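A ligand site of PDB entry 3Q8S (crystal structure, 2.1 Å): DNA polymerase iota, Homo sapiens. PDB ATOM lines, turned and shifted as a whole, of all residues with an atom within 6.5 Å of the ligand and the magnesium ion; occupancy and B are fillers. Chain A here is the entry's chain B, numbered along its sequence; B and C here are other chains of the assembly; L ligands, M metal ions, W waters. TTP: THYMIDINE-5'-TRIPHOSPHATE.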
ATOM      1  N   ASP A  34      26.021   9.335 -12.548  1.00  0.00           N
ATOM      2  CA  ASP A  34      26.437   8.049 -13.084  1.00  0.00           C
ATOM      3  C   ASP A  34      25.187   7.243 -13.432  1.00  0.00           C
ATOM      4  O   ASP A  34      24.446   6.829 -12.549  1.00  0.00           O
ATOM      5  CB  ASP A  34      27.260   7.297 -12.020  1.00  0.00           C
ATOM      6  CG  ASP A  34      27.956   6.075 -12.589  1.00  0.00           C
ATOM      7  OD1 ASP A  34      27.500   5.576 -13.633  1.00  0.00           O
ATOM      8  OD2 ASP A  34      28.954   5.612 -12.009  1.00  0.00           O
ATOM      9  N   LEU A  35      24.957   7.035 -14.731  1.00  0.00           N
ATOM     10  CA  LEU A  35      23.705   6.410 -15.181  1.00  0.00           C
ATOM     11  C   LEU A  35      23.659   4.945 -14.826  1.00  0.00           C
ATOM     12  O   LEU A  35      24.671   4.281 -14.822  1.00  0.00           O
ATOM     13  CB  LEU A  35      23.562   6.561 -16.702  1.00  0.00           C
ATOM     14  CG  LEU A  35      22.887   7.824 -17.202  1.00  0.00           C
ATOM     15  CD1 LEU A  35      23.250   8.998 -16.355  1.00  0.00           C
ATOM     16  CD2 LEU A  35      23.215   8.111 -18.674  1.00  0.00           C
ATOM     17  N   ASP A  36      22.471   4.438 -14.526  1.00  0.00           N
ATOM     18  CA  ASP A  36      22.324   3.023 -14.245  1.00  0.00           C
ATOM     19  C   ASP A  36      22.257   2.015 -15.388  1.00  0.00           C
ATOM     20  O   ASP A  36      21.397   2.124 -16.273  1.00  0.00           O
ATOM     21  CB  ASP A  36      20.952   2.740 -13.618  1.00  0.00           C
ATOM     22  CG  ASP A  36      20.756   3.450 -12.293  1.00  0.00           C
ATOM     23  OD1 ASP A  36      21.736   3.579 -11.508  1.00  0.00           O
ATOM     24  OD2 ASP A  36      19.626   3.869 -12.023  1.00  0.00           O
ATOM     25  N   CYS A  37      23.176   1.036 -15.362  1.00  0.00           N
ATOM     26  CA  CYS A  37      23.477   0.103 -16.439  1.00  0.00           C
ATOM     27  C   CYS A  37      23.256   0.720 -17.828  1.00  0.00           C
ATOM     28  O   CYS A  37      22.423   0.253 -18.591  1.00  0.00           O
ATOM     29  CB  CYS A  37      22.632  -1.164 -16.267  1.00  0.00           C
ATOM     30  SG  CYS A  37      20.865  -0.869 -16.081  1.00  0.00           S
ATOM     31  N   PHE A  38      24.044   1.739 -18.144  1.00  0.00           N
ATOM     32  CA  PHE A  38      23.757   2.636 -19.268  1.00  0.00           C
ATOM     33  C   PHE A  38      23.261   1.978 -20.577  1.00  0.00           C
ATOM     34  O   PHE A  38      22.139   2.231 -20.996  1.00  0.00           O
ATOM     35  CB  PHE A  38      24.933   3.563 -19.566  1.00  0.00           C
ATOM     36  CG  PHE A  38      24.628   4.589 -20.625  1.00  0.00           C
ATOM     37  CD1 PHE A  38      23.466   5.333 -20.563  1.00  0.00           C
ATOM     38  CD2 PHE A  38      25.501   4.802 -21.672  1.00  0.00           C
ATOM     39  CE1 PHE A  38      23.170   6.280 -21.544  1.00  0.00           C
ATOM     40  CE2 PHE A  38      25.220   5.742 -22.645  1.00  0.00           C
ATOM     41  CZ  PHE A  38      24.061   6.488 -22.574  1.00  0.00           C
ATOM     42  N   TYR A  39      24.102   1.169 -21.216  1.00  0.00           N
ATOM     43  CA  TYR A  39      23.718   0.578 -22.512  1.00  0.00           C
ATOM     44  C   TYR A  39      22.408  -0.196 -22.395  1.00  0.00           C
ATOM     45  O   TYR A  39      21.501  -0.024 -23.202  1.00  0.00           O
ATOM     46  CB  TYR A  39      24.802  -0.361 -23.044  1.00  0.00           C
ATOM     47  CG  TYR A  39      26.064   0.313 -23.512  1.00  0.00           C
ATOM     48  CD1 TYR A  39      27.091  -0.445 -24.063  1.00  0.00           C
ATOM     49  CD2 TYR A  39      26.264   1.684 -23.371  1.00  0.00           C
ATOM     50  CE1 TYR A  39      28.269   0.154 -24.497  1.00  0.00           C
ATOM     51  CE2 TYR A  39      27.443   2.295 -23.798  1.00  0.00           C
ATOM     52  CZ  TYR A  39      28.440   1.509 -24.354  1.00  0.00           C
ATOM     53  OH  TYR A  39      29.615   2.078 -24.781  1.00  0.00           O
ATOM     54  N   ALA A  40      22.326  -1.041 -21.373  1.00  0.00           N
ATOM     55  CA  ALA A  40      21.139  -1.845 -21.140  1.00  0.00           C
ATOM     56  C   ALA A  40      19.899  -0.957 -20.964  1.00  0.00           C
ATOM     57  O   ALA A  40      18.833  -1.273 -21.477  1.00  0.00           O
ATOM     58  CB  ALA A  40      21.317  -2.754 -19.934  1.00  0.00           C
ATOM     59  N   GLN A  59      29.007  -7.475 -27.007  1.00  0.00           N
ATOM     60  CA  GLN A  59      29.943  -6.994 -28.002  1.00  0.00           C
ATOM     61  C   GLN A  59      30.920  -8.129 -28.296  1.00  0.00           C
ATOM     62  O   GLN A  59      31.738  -8.492 -27.462  1.00  0.00           O
ATOM     63  CB  GLN A  59      30.678  -5.748 -27.488  1.00  0.00           C
ATOM     64  CG  GLN A  59      29.817  -4.489 -27.442  1.00  0.00           C
ATOM     65  CD  GLN A  59      30.549  -3.292 -26.841  1.00  0.00           C
ATOM     66  OE1 GLN A  59      31.514  -3.462 -26.107  1.00  0.00           O
ATOM     67  NE2 GLN A  59      30.087  -2.083 -27.165  1.00  0.00           N
ATOM     68  N   VAL A  64      29.217  -6.686 -22.092  1.00  0.00           N
ATOM     69  CA  VAL A  64      29.840  -5.490 -21.551  1.00  0.00           C
ATOM     70  C   VAL A  64      29.099  -4.970 -20.326  1.00  0.00           C
ATOM     71  O   VAL A  64      29.720  -4.501 -19.374  1.00  0.00           O
ATOM     72  CB  VAL A  64      30.016  -4.384 -22.616  1.00  0.00           C
ATOM     73  CG1 VAL A  64      30.786  -4.941 -23.779  1.00  0.00           C
ATOM     74  CG2 VAL A  64      28.668  -3.835 -23.086  1.00  0.00           C
ATOM     75  N   THR A  65      27.781  -5.064 -20.348  1.00  0.00           N
ATOM     76  CA  THR A  65      26.971  -4.692 -19.198  1.00  0.00           C
ATOM     77  C   THR A  65      25.609  -5.398 -19.250  1.00  0.00           C
ATOM     78  O   THR A  65      25.235  -5.959 -20.275  1.00  0.00           O
ATOM     79  CB  THR A  65      26.762  -3.156 -19.105  1.00  0.00           C
ATOM     80  OG1 THR A  65      26.269  -2.811 -17.808  1.00  0.00           O
ATOM     81  CG2 THR A  65      25.795  -2.651 -20.166  1.00  0.00           C
ATOM     82  N   CYS A  66      24.894  -5.362 -18.135  1.00  0.00           N
ATOM     83  CA  CYS A  66      23.580  -5.994 -18.025  1.00  0.00           C
ATOM     84  C   CYS A  66      22.710  -5.197 -17.062  1.00  0.00           C
ATOM     85  O   CYS A  66      23.230  -4.475 -16.215  1.00  0.00           O
ATOM     86  CB  CYS A  66      23.735  -7.427 -17.519  1.00  0.00           C
ATOM     87  SG  CYS A  66      24.611  -7.570 -15.933  1.00  0.00           S
ATOM     88  N   TYR A  68      19.796  -4.693 -13.932  1.00  0.00           N
ATOM     89  CA  TYR A  68      19.863  -5.156 -12.546  1.00  0.00           C
ATOM     90  C   TYR A  68      19.080  -6.431 -12.296  1.00  0.00           C
ATOM     91  O   TYR A  68      19.335  -7.150 -11.328  1.00  0.00           O
ATOM     92  CB  TYR A  68      19.480  -4.030 -11.578  1.00  0.00           C
ATOM     93  CG  TYR A  68      20.621  -3.064 -11.400  1.00  0.00           C
ATOM     94  CD1 TYR A  68      20.855  -2.061 -12.322  1.00  0.00           C
ATOM     95  CD2 TYR A  68      21.491  -3.174 -10.313  1.00  0.00           C
ATOM     96  CE1 TYR A  68      21.909  -1.181 -12.183  1.00  0.00           C
ATOM     97  CE2 TYR A  68      22.554  -2.300 -10.154  1.00  0.00           C
ATOM     98  CZ  TYR A  68      22.751  -1.295 -11.086  1.00  0.00           C
ATOM     99  OH  TYR A  68      23.802  -0.417 -10.956  1.00  0.00           O
ATOM    100  N   ARG A  71      21.906  -8.886 -12.934  1.00  0.00           N
ATOM    101  CA  ARG A  71      22.933  -8.949 -11.899  1.00  0.00           C
ATOM    102  C   ARG A  71      22.420  -9.714 -10.696  1.00  0.00           C
ATOM    103  O   ARG A  71      23.187 -10.350  -9.971  1.00  0.00           O
ATOM    104  CB  ARG A  71      23.395  -7.538 -11.500  1.00  0.00           C
ATOM    105  CG  ARG A  71      23.922  -6.725 -12.675  1.00  0.00           C
ATOM    106  CD  ARG A  71      24.397  -5.332 -12.276  1.00  0.00           C
ATOM    107  NE  ARG A  71      24.595  -4.495 -13.453  1.00  0.00           N
ATOM    108  CZ  ARG A  71      25.218  -3.312 -13.448  1.00  0.00           C
ATOM    109  NH1 ARG A  71      25.706  -2.815 -12.317  1.00  0.00           N
ATOM    110  NH2 ARG A  71      25.340  -2.629 -14.578  1.00  0.00           N
ATOM    111  N   LYS A  77      29.375  -7.440 -14.998  1.00  0.00           N
ATOM    112  CA  LYS A  77      29.871  -6.613 -16.101  1.00  0.00           C
ATOM    113  C   LYS A  77      31.090  -7.252 -16.752  1.00  0.00           C
ATOM    114  O   LYS A  77      31.961  -7.790 -16.082  1.00  0.00           O
ATOM    115  CB  LYS A  77      30.237  -5.210 -15.614  1.00  0.00           C
ATOM    116  CG  LYS A  77      29.076  -4.424 -15.035  1.00  0.00           C
ATOM    117  CD  LYS A  77      29.496  -2.972 -14.791  1.00  0.00           C
ATOM    118  CE  LYS A  77      29.156  -2.507 -13.377  1.00  0.00           C
ATOM    119  NZ  LYS A  77      29.656  -1.129 -13.124  1.00  0.00           N
ATOM    120  N   LEU A  78      31.147  -7.178 -18.088  1.00  0.00           N
ATOM    121  CA  LEU A  78      32.304  -7.658 -18.837  1.00  0.00           C
ATOM    122  C   LEU A  78      32.523  -9.174 -18.722  1.00  0.00           C
ATOM    123  O   LEU A  78      33.656  -9.647 -18.863  1.00  0.00           O
ATOM    124  CB  LEU A  78      33.574  -6.919 -18.407  1.00  0.00           C
ATOM    125  CG  LEU A  78      33.563  -5.393 -18.540  1.00  0.00           C
ATOM    126  CD1 LEU A  78      34.616  -4.768 -17.637  1.00  0.00           C
ATOM    127  CD2 LEU A  78      33.774  -4.971 -19.979  1.00  0.00           C
ATOM    128  N   LEU A  99      27.714   1.931 -31.350  1.00  0.00           N
ATOM    129  CA  LEU A  99      27.525   2.804 -30.200  1.00  0.00           C
ATOM    130  C   LEU A  99      26.641   4.010 -30.501  1.00  0.00           C
ATOM    131  O   LEU A  99      26.460   4.866 -29.630  1.00  0.00           O
ATOM    132  CB  LEU A  99      28.868   3.321 -29.694  1.00  0.00           C
ATOM    133  CG  LEU A  99      29.928   2.306 -29.245  1.00  0.00           C
ATOM    134  CD1 LEU A  99      31.030   3.018 -28.463  1.00  0.00           C
ATOM    135  CD2 LEU A  99      29.297   1.207 -28.417  1.00  0.00           C
ATOM    136  N   PHE A 125      30.892   7.536 -21.567  1.00  0.00           N
ATOM    137  CA  PHE A 125      29.582   7.855 -22.120  1.00  0.00           C
ATOM    138  C   PHE A 125      28.503   8.092 -21.087  1.00  0.00           C
ATOM    139  O   PHE A 125      27.463   8.686 -21.401  1.00  0.00           O
ATOM    140  CB  PHE A 125      29.112   6.774 -23.101  1.00  0.00           C
ATOM    141  CG  PHE A 125      29.667   6.914 -24.489  1.00  0.00           C
ATOM    142  CD1 PHE A 125      30.659   7.826 -24.765  1.00  0.00           C
ATOM    143  CD2 PHE A 125      29.179   6.130 -25.537  1.00  0.00           C
ATOM    144  CE1 PHE A 125      31.181   7.954 -26.042  1.00  0.00           C
ATOM    145  CE2 PHE A 125      29.682   6.255 -26.807  1.00  0.00           C
ATOM    146  CZ  PHE A 125      30.681   7.171 -27.065  1.00  0.00           C
ATOM    147  N   ASP A 126      28.705   7.623 -19.863  1.00  0.00           N
ATOM    148  CA  ASP A 126      27.586   7.673 -18.929  1.00  0.00           C
ATOM    149  C   ASP A 126      27.846   8.388 -17.595  1.00  0.00           C
ATOM    150  O   ASP A 126      27.016   8.319 -16.690  1.00  0.00           O
ATOM    151  CB  ASP A 126      27.039   6.273 -18.678  1.00  0.00           C
ATOM    152  CG  ASP A 126      27.602   5.638 -17.422  1.00  0.00           C
ATOM    153  OD1 ASP A 126      26.793   5.158 -16.609  1.00  0.00           O
ATOM    154  OD2 ASP A 126      28.839   5.632 -17.255  1.00  0.00           O
ATOM    155  N   GLU A 127      28.961   9.091 -17.482  1.00  0.00           N
ATOM    156  CA  GLU A 127      29.252   9.839 -16.252  1.00  0.00           C
ATOM    157  C   GLU A 127      29.549  11.305 -16.541  1.00  0.00           C
ATOM    158  O   GLU A 127      30.148  11.619 -17.560  1.00  0.00           O
ATOM    159  CB  GLU A 127      30.419   9.210 -15.490  1.00  0.00           C
ATOM    160  CG  GLU A 127      30.082   7.863 -14.880  1.00  0.00           C
ATOM    161  CD  GLU A 127      31.297   7.140 -14.351  1.00  0.00           C
ATOM    162  OE1 GLU A 127      32.195   7.820 -13.784  1.00  0.00           O
ATOM    163  OE2 GLU A 127      31.365   5.907 -14.492  1.00  0.00           O
ATOM    164  N   LYS A 214      23.170   2.019  -4.867  1.00  0.00           N
ATOM    165  CA  LYS A 214      22.781   1.786  -6.257  1.00  0.00           C
ATOM    166  C   LYS A 214      21.695   0.727  -6.296  1.00  0.00           C
ATOM    167  O   LYS A 214      21.619  -0.102  -5.397  1.00  0.00           O
ATOM    168  CB  LYS A 214      23.970   1.253  -7.060  1.00  0.00           C
ATOM    169  CG  LYS A 214      24.962   2.300  -7.483  1.00  0.00           C
ATOM    170  CD  LYS A 214      26.295   1.651  -7.859  1.00  0.00           C
ATOM    171  CE  LYS A 214      26.091   0.529  -8.867  1.00  0.00           C
ATOM    172  NZ  LYS A 214      27.376   0.066  -9.470  1.00  0.00           N
ATOM    173  N   PRO A 215      20.854   0.734  -7.348  1.00  0.00           N
ATOM    174  CA  PRO A 215      20.858   1.730  -8.429  1.00  0.00           C
ATOM    175  C   PRO A 215      19.899   2.889  -8.135  1.00  0.00           C
ATOM    176  O   PRO A 215      19.182   2.867  -7.138  1.00  0.00           O
ATOM    177  CB  PRO A 215      20.347   0.940  -9.630  1.00  0.00           C
ATOM    178  CG  PRO A 215      19.406  -0.052  -9.042  1.00  0.00           C
ATOM    179  CD  PRO A 215      19.970  -0.402  -7.663  1.00  0.00           C
ATOM    180  P   8OG B   4      38.580  -7.720 -28.240  1.00  0.00           P
ATOM    181  OP1 8OG B   4      38.970  -8.611 -29.377  1.00  0.00           O
ATOM    182  OP2 8OG B   4      38.842  -8.168 -26.814  1.00  0.00           O
ATOM    183  O5' 8OG B   4      37.018  -7.388 -28.388  1.00  0.00           O
ATOM    184  C5' 8OG B   4      36.217  -7.229 -27.217  1.00  0.00           C
ATOM    185  C4' 8OG B   4      35.036  -6.296 -27.479  1.00  0.00           C
ATOM    186  O4' 8OG B   4      34.670  -5.686 -26.248  1.00  0.00           O
ATOM    187  C3' 8OG B   4      35.341  -5.185 -28.481  1.00  0.00           C
ATOM    188  O3' 8OG B   4      34.230  -5.101 -29.384  1.00  0.00           O
ATOM    189  C2' 8OG B   4      35.429  -3.915 -27.636  1.00  0.00           C
ATOM    190  C1' 8OG B   4      34.793  -4.264 -26.296  1.00  0.00           C
ATOM    191  N9  8OG B   4      35.508  -3.741 -25.097  1.00  0.00           N
ATOM    192  C8  8OG B   4      34.967  -3.064 -24.079  1.00  0.00           C
ATOM    193  N7  8OG B   4      35.776  -2.685 -23.096  1.00  0.00           N
ATOM    194  C5  8OG B   4      36.962  -3.170 -23.478  1.00  0.00           C
ATOM    195  C6  8OG B   4      38.318  -3.143 -22.884  1.00  0.00           C
ATOM    196  O6  8OG B   4      38.499  -2.572 -21.796  1.00  0.00           O
ATOM    197  N1  8OG B   4      39.308  -3.740 -23.554  1.00  0.00           N
ATOM    198  C2  8OG B   4      39.111  -4.358 -24.735  1.00  0.00           C
ATOM    199  N2  8OG B   4      40.180  -4.949 -25.335  1.00  0.00           N
ATOM    200  N3  8OG B   4      37.899  -4.428 -25.335  1.00  0.00           N
ATOM    201  C4  8OG B   4      36.798  -3.859 -24.774  1.00  0.00           C
ATOM    202  O8  8OG B   4      33.755  -2.757 -24.049  1.00  0.00           O
ATOM    203  P    DG B   5      34.278  -4.371 -30.811  1.00  0.00           P
ATOM    204  OP1  DG B   5      33.138  -4.751 -31.672  1.00  0.00           O
ATOM    205  OP2  DG B   5      35.668  -4.444 -31.283  1.00  0.00           O
ATOM    206  O5'  DG B   5      33.959  -2.887 -30.337  1.00  0.00           O
ATOM    207  C5'  DG B   5      32.624  -2.404 -30.184  1.00  0.00           C
ATOM    208  C4'  DG B   5      32.657  -0.946 -29.759  1.00  0.00           C
ATOM    209  O4'  DG B   5      33.302  -0.857 -28.467  1.00  0.00           O
ATOM    210  C3'  DG B   5      33.492  -0.053 -30.677  1.00  0.00           C
ATOM    211  O3'  DG B   5      32.925   1.230 -30.756  1.00  0.00           O
ATOM    212  C2'  DG B   5      34.836   0.017 -29.981  1.00  0.00           C
ATOM    213  C1'  DG B   5      34.299   0.123 -28.555  1.00  0.00           C
ATOM    214  N9   DG B   5      35.294  -0.081 -27.523  1.00  0.00           N
ATOM    215  C8   DG B   5      36.457  -0.814 -27.576  1.00  0.00           C
ATOM    216  N7   DG B   5      37.142  -0.773 -26.460  1.00  0.00           N
ATOM    217  C5   DG B   5      36.364   0.026 -25.624  1.00  0.00           C
ATOM    218  C6   DG B   5      36.589   0.424 -24.288  1.00  0.00           C
ATOM    219  O6   DG B   5      37.542   0.139 -23.548  1.00  0.00           O
ATOM    220  N1   DG B   5      35.559   1.240 -23.835  1.00  0.00           N
ATOM    221  C2   DG B   5      34.458   1.620 -24.556  1.00  0.00           C
ATOM    222  N2   DG B   5      33.573   2.420 -23.921  1.00  0.00           N
ATOM    223  N3   DG B   5      34.232   1.245 -25.799  1.00  0.00           N
ATOM    224  C4   DG B   5      35.231   0.462 -26.261  1.00  0.00           C
ATOM    225  P    DC C   7      36.389   4.277 -14.222  1.00  0.00           P
ATOM    226  OP1  DC C   7      35.675   4.408 -12.945  1.00  0.00           O
ATOM    227  OP2  DC C   7      37.343   3.162 -14.480  1.00  0.00           O
ATOM    228  O5'  DC C   7      35.303   4.192 -15.421  1.00  0.00           O
ATOM    229  C5'  DC C   7      34.354   5.249 -15.582  1.00  0.00           C
ATOM    230  C4'  DC C   7      33.543   5.047 -16.848  1.00  0.00           C
ATOM    231  O4'  DC C   7      34.380   5.277 -18.016  1.00  0.00           O
ATOM    232  C3'  DC C   7      32.994   3.643 -17.069  1.00  0.00           C
ATOM    233  C2'  DC C   7      32.745   3.669 -18.583  1.00  0.00           C
ATOM    234  C1'  DC C   7      33.963   4.445 -19.067  1.00  0.00           C
ATOM    235  N1   DC C   7      35.076   3.539 -19.477  1.00  0.00           N
ATOM    236  C2   DC C   7      35.008   3.016 -20.764  1.00  0.00           C
ATOM    237  O2   DC C   7      34.050   3.345 -21.468  1.00  0.00           O
ATOM    238  N3   DC C   7      35.987   2.183 -21.186  1.00  0.00           N
ATOM    239  C4   DC C   7      36.987   1.890 -20.352  1.00  0.00           C
ATOM    240  N4   DC C   7      37.936   1.058 -20.797  1.00  0.00           N
ATOM    241  C5   DC C   7      37.066   2.409 -19.036  1.00  0.00           C
ATOM    242  C6   DC C   7      36.093   3.230 -18.634  1.00  0.00           C
HETATM  243  PA  TTP L   1      29.826   1.799 -16.052  1.00  0.00           P
HETATM  244  O1A TTP L   1      31.165   1.440 -15.468  1.00  0.00           O
HETATM  245  O2A TTP L   1      29.384   3.153 -15.585  1.00  0.00           O
HETATM  246  O3A TTP L   1      28.733   0.685 -15.667  1.00  0.00           O
HETATM  247  PB  TTP L   1      27.178   0.754 -16.085  1.00  0.00           P
HETATM  248  O1B TTP L   1      26.695   2.161 -16.293  1.00  0.00           O
HETATM  249  O2B TTP L   1      26.963  -0.082 -17.322  1.00  0.00           O
HETATM  250  O3B TTP L   1      26.414   0.052 -14.865  1.00  0.00           O
HETATM  251  PG  TTP L   1      26.352   0.688 -13.386  1.00  0.00           P
HETATM  252  O1G TTP L   1      24.920   0.697 -12.940  1.00  0.00           O
HETATM  253  O2G TTP L   1      26.902   2.085 -13.368  1.00  0.00           O
HETATM  254  O3G TTP L   1      27.158  -0.193 -12.482  1.00  0.00           O
HETATM  255  O5' TTP L   1      29.908   1.758 -17.662  1.00  0.00           O
HETATM  256  C5' TTP L   1      29.167   2.678 -18.456  1.00  0.00           C
HETATM  257  C4' TTP L   1      28.990   2.105 -19.857  1.00  0.00           C
HETATM  258  O4' TTP L   1      30.243   2.096 -20.554  1.00  0.00           O
HETATM  259  C3' TTP L   1      28.505   0.671 -19.803  1.00  0.00           C
HETATM  260  O3' TTP L   1      27.115   0.613 -20.120  1.00  0.00           O
HETATM  261  C2' TTP L   1      29.326  -0.083 -20.823  1.00  0.00           C
HETATM  262  C1' TTP L   1      30.407   0.875 -21.278  1.00  0.00           C
HETATM  263  N1  TTP L   1      31.723   0.277 -21.035  1.00  0.00           N
HETATM  264  C2  TTP L   1      32.414  -0.353 -22.092  1.00  0.00           C
HETATM  265  O2  TTP L   1      31.882  -0.386 -23.229  1.00  0.00           O
HETATM  266  N3  TTP L   1      33.615  -0.922 -21.913  1.00  0.00           N
HETATM  267  C4  TTP L   1      34.194  -0.902 -20.713  1.00  0.00           C
HETATM  268  O4  TTP L   1      35.312  -1.427 -20.537  1.00  0.00           O
HETATM  269  C5  TTP L   1      33.502  -0.241 -19.588  1.00  0.00           C
HETATM  270  C5M TTP L   1      34.149  -0.215 -18.229  1.00  0.00           C
HETATM  271  C6  TTP L   1      32.262   0.334 -19.809  1.00  0.00           C
HETATM  272 MG    MG M   1      26.819   3.794 -14.816  1.00  0.00          MG
HETATM  273  O   HOH W   1      37.019  -1.295 -17.718  1.00  0.00           O
HETATM  274  O   HOH W   2      23.973   2.414 -11.025  1.00  0.00           O
HETATM  275  O   HOH W   3      31.462   0.450 -25.704  1.00  0.00           O
HETATM  276  O   HOH W   4      29.361   2.753 -11.902  1.00  0.00           O
HETATM  277  O   HOH W   5      25.700   4.462 -12.183  1.00  0.00           O
HETATM  278  O   HOH W   6      32.774   2.140 -13.606  1.00  0.00           O
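The side-chain amino group of Lys 77 is in salt-bridge range of an oxygen (O3G) of the ligand. O1G of the ligand is in hydrogen-bond range of OH of Tyr 68, at 2.5 Å. O8 of 8OG 4 of chain B sits at hydrogen-bond distance from a nitrogen (N3) of the ligand (2.8 Å). The guanidinium group (NH1) of Arg 71 lies within salt-bridge range of an oxygen (O3G) of the ligand. An oxygen (O3') of the ligand sits at hydrogen-bond distance from the backbone NH of Tyr 39 (3.3 Å). N1 of DG 5 of chain B is in hydrogen-bond range of a nitrogen (N3) of the ligand, at 3.5 Å. NZ of Lys 214 is in salt-bridge range of O3G of the ligand (3.0 Å). N of Cys 37 is in hydrogen-bond range of O1G of the ligand, at 3.0 Å. The side-chain hydroxyl (OG1) of Thr 65 is in hydrogen-bond range of an oxygen (O2B) of the ligand, 2.9 Å away. O1B of the ligand lies close to N of Phe 38 (3.3 Å).
The backbone NH (N) of Leu 78 sits at hydrogen-bond distance from the backbone carbonyl oxygen (O) of Val 64. OG1 of Thr 65 is in hydrogen-bond range of NH2 of Arg 71 (3.4 Å). O8 of 8OG 4 of chain B sits close to the side-chain amide oxygen of Gln 59, at 3.1 Å. OH of Tyr 68 lies within hydrogen-bond range of NH1 of Arg 71. NE of Arg 71 sits at hydrogen-bond distance from O of Cys 66, 3.1 Å away. O2 of DC 7 of chain C sits close to N2 of DG 5 of chain B (2.7 Å).
Asp 36 touches the ligand (CA to O1G, 3.7 Å). CD2 of Leu 78 touches O4 of the ligand (3.9 Å). Glu 127 touches the ligand. C3' of DC 7 of chain C touches O1A of the ligand, 3.3 Å away. Of the 24 residues printed, 17 come within 4 Å of the ligand.
Three residues have an atom within 4 Å of the magnesium ion: Asp 34, Leu 35 and Asp 126.
The magnesium ion is bound by the backbone carbonyl oxygen (O) of Leu 35 (2.2 Å), an oxygen (O1B) of the ligand (2.2 Å), an oxygen (O2G) of the ligand (2.2 Å), the side-chain carboxylate (OD1) of Asp 34 (2.2 Å) and the side-chain carboxylate (OD1) of Asp 126 (2.3 Å). The magnesium ion has five donor atoms within binding distance. Slightly farther from the magnesium ion lies O2A of the ligand (2.8 Å).
Water W3 lies within hydrogen-bond range of OH of Tyr 39 (2.6 Å), O2 of the ligand (2.6 Å), N3 of DG 5 of chain B (2.9 Å) and NE2 of Gln 59 (3.2 Å). Water W2 lies within hydrogen-bond range of the side-chain carboxylate (OD1) of Asp 36, an oxygen (O1G) of the ligand and the side-chain hydroxyl (OH) of Tyr 68.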
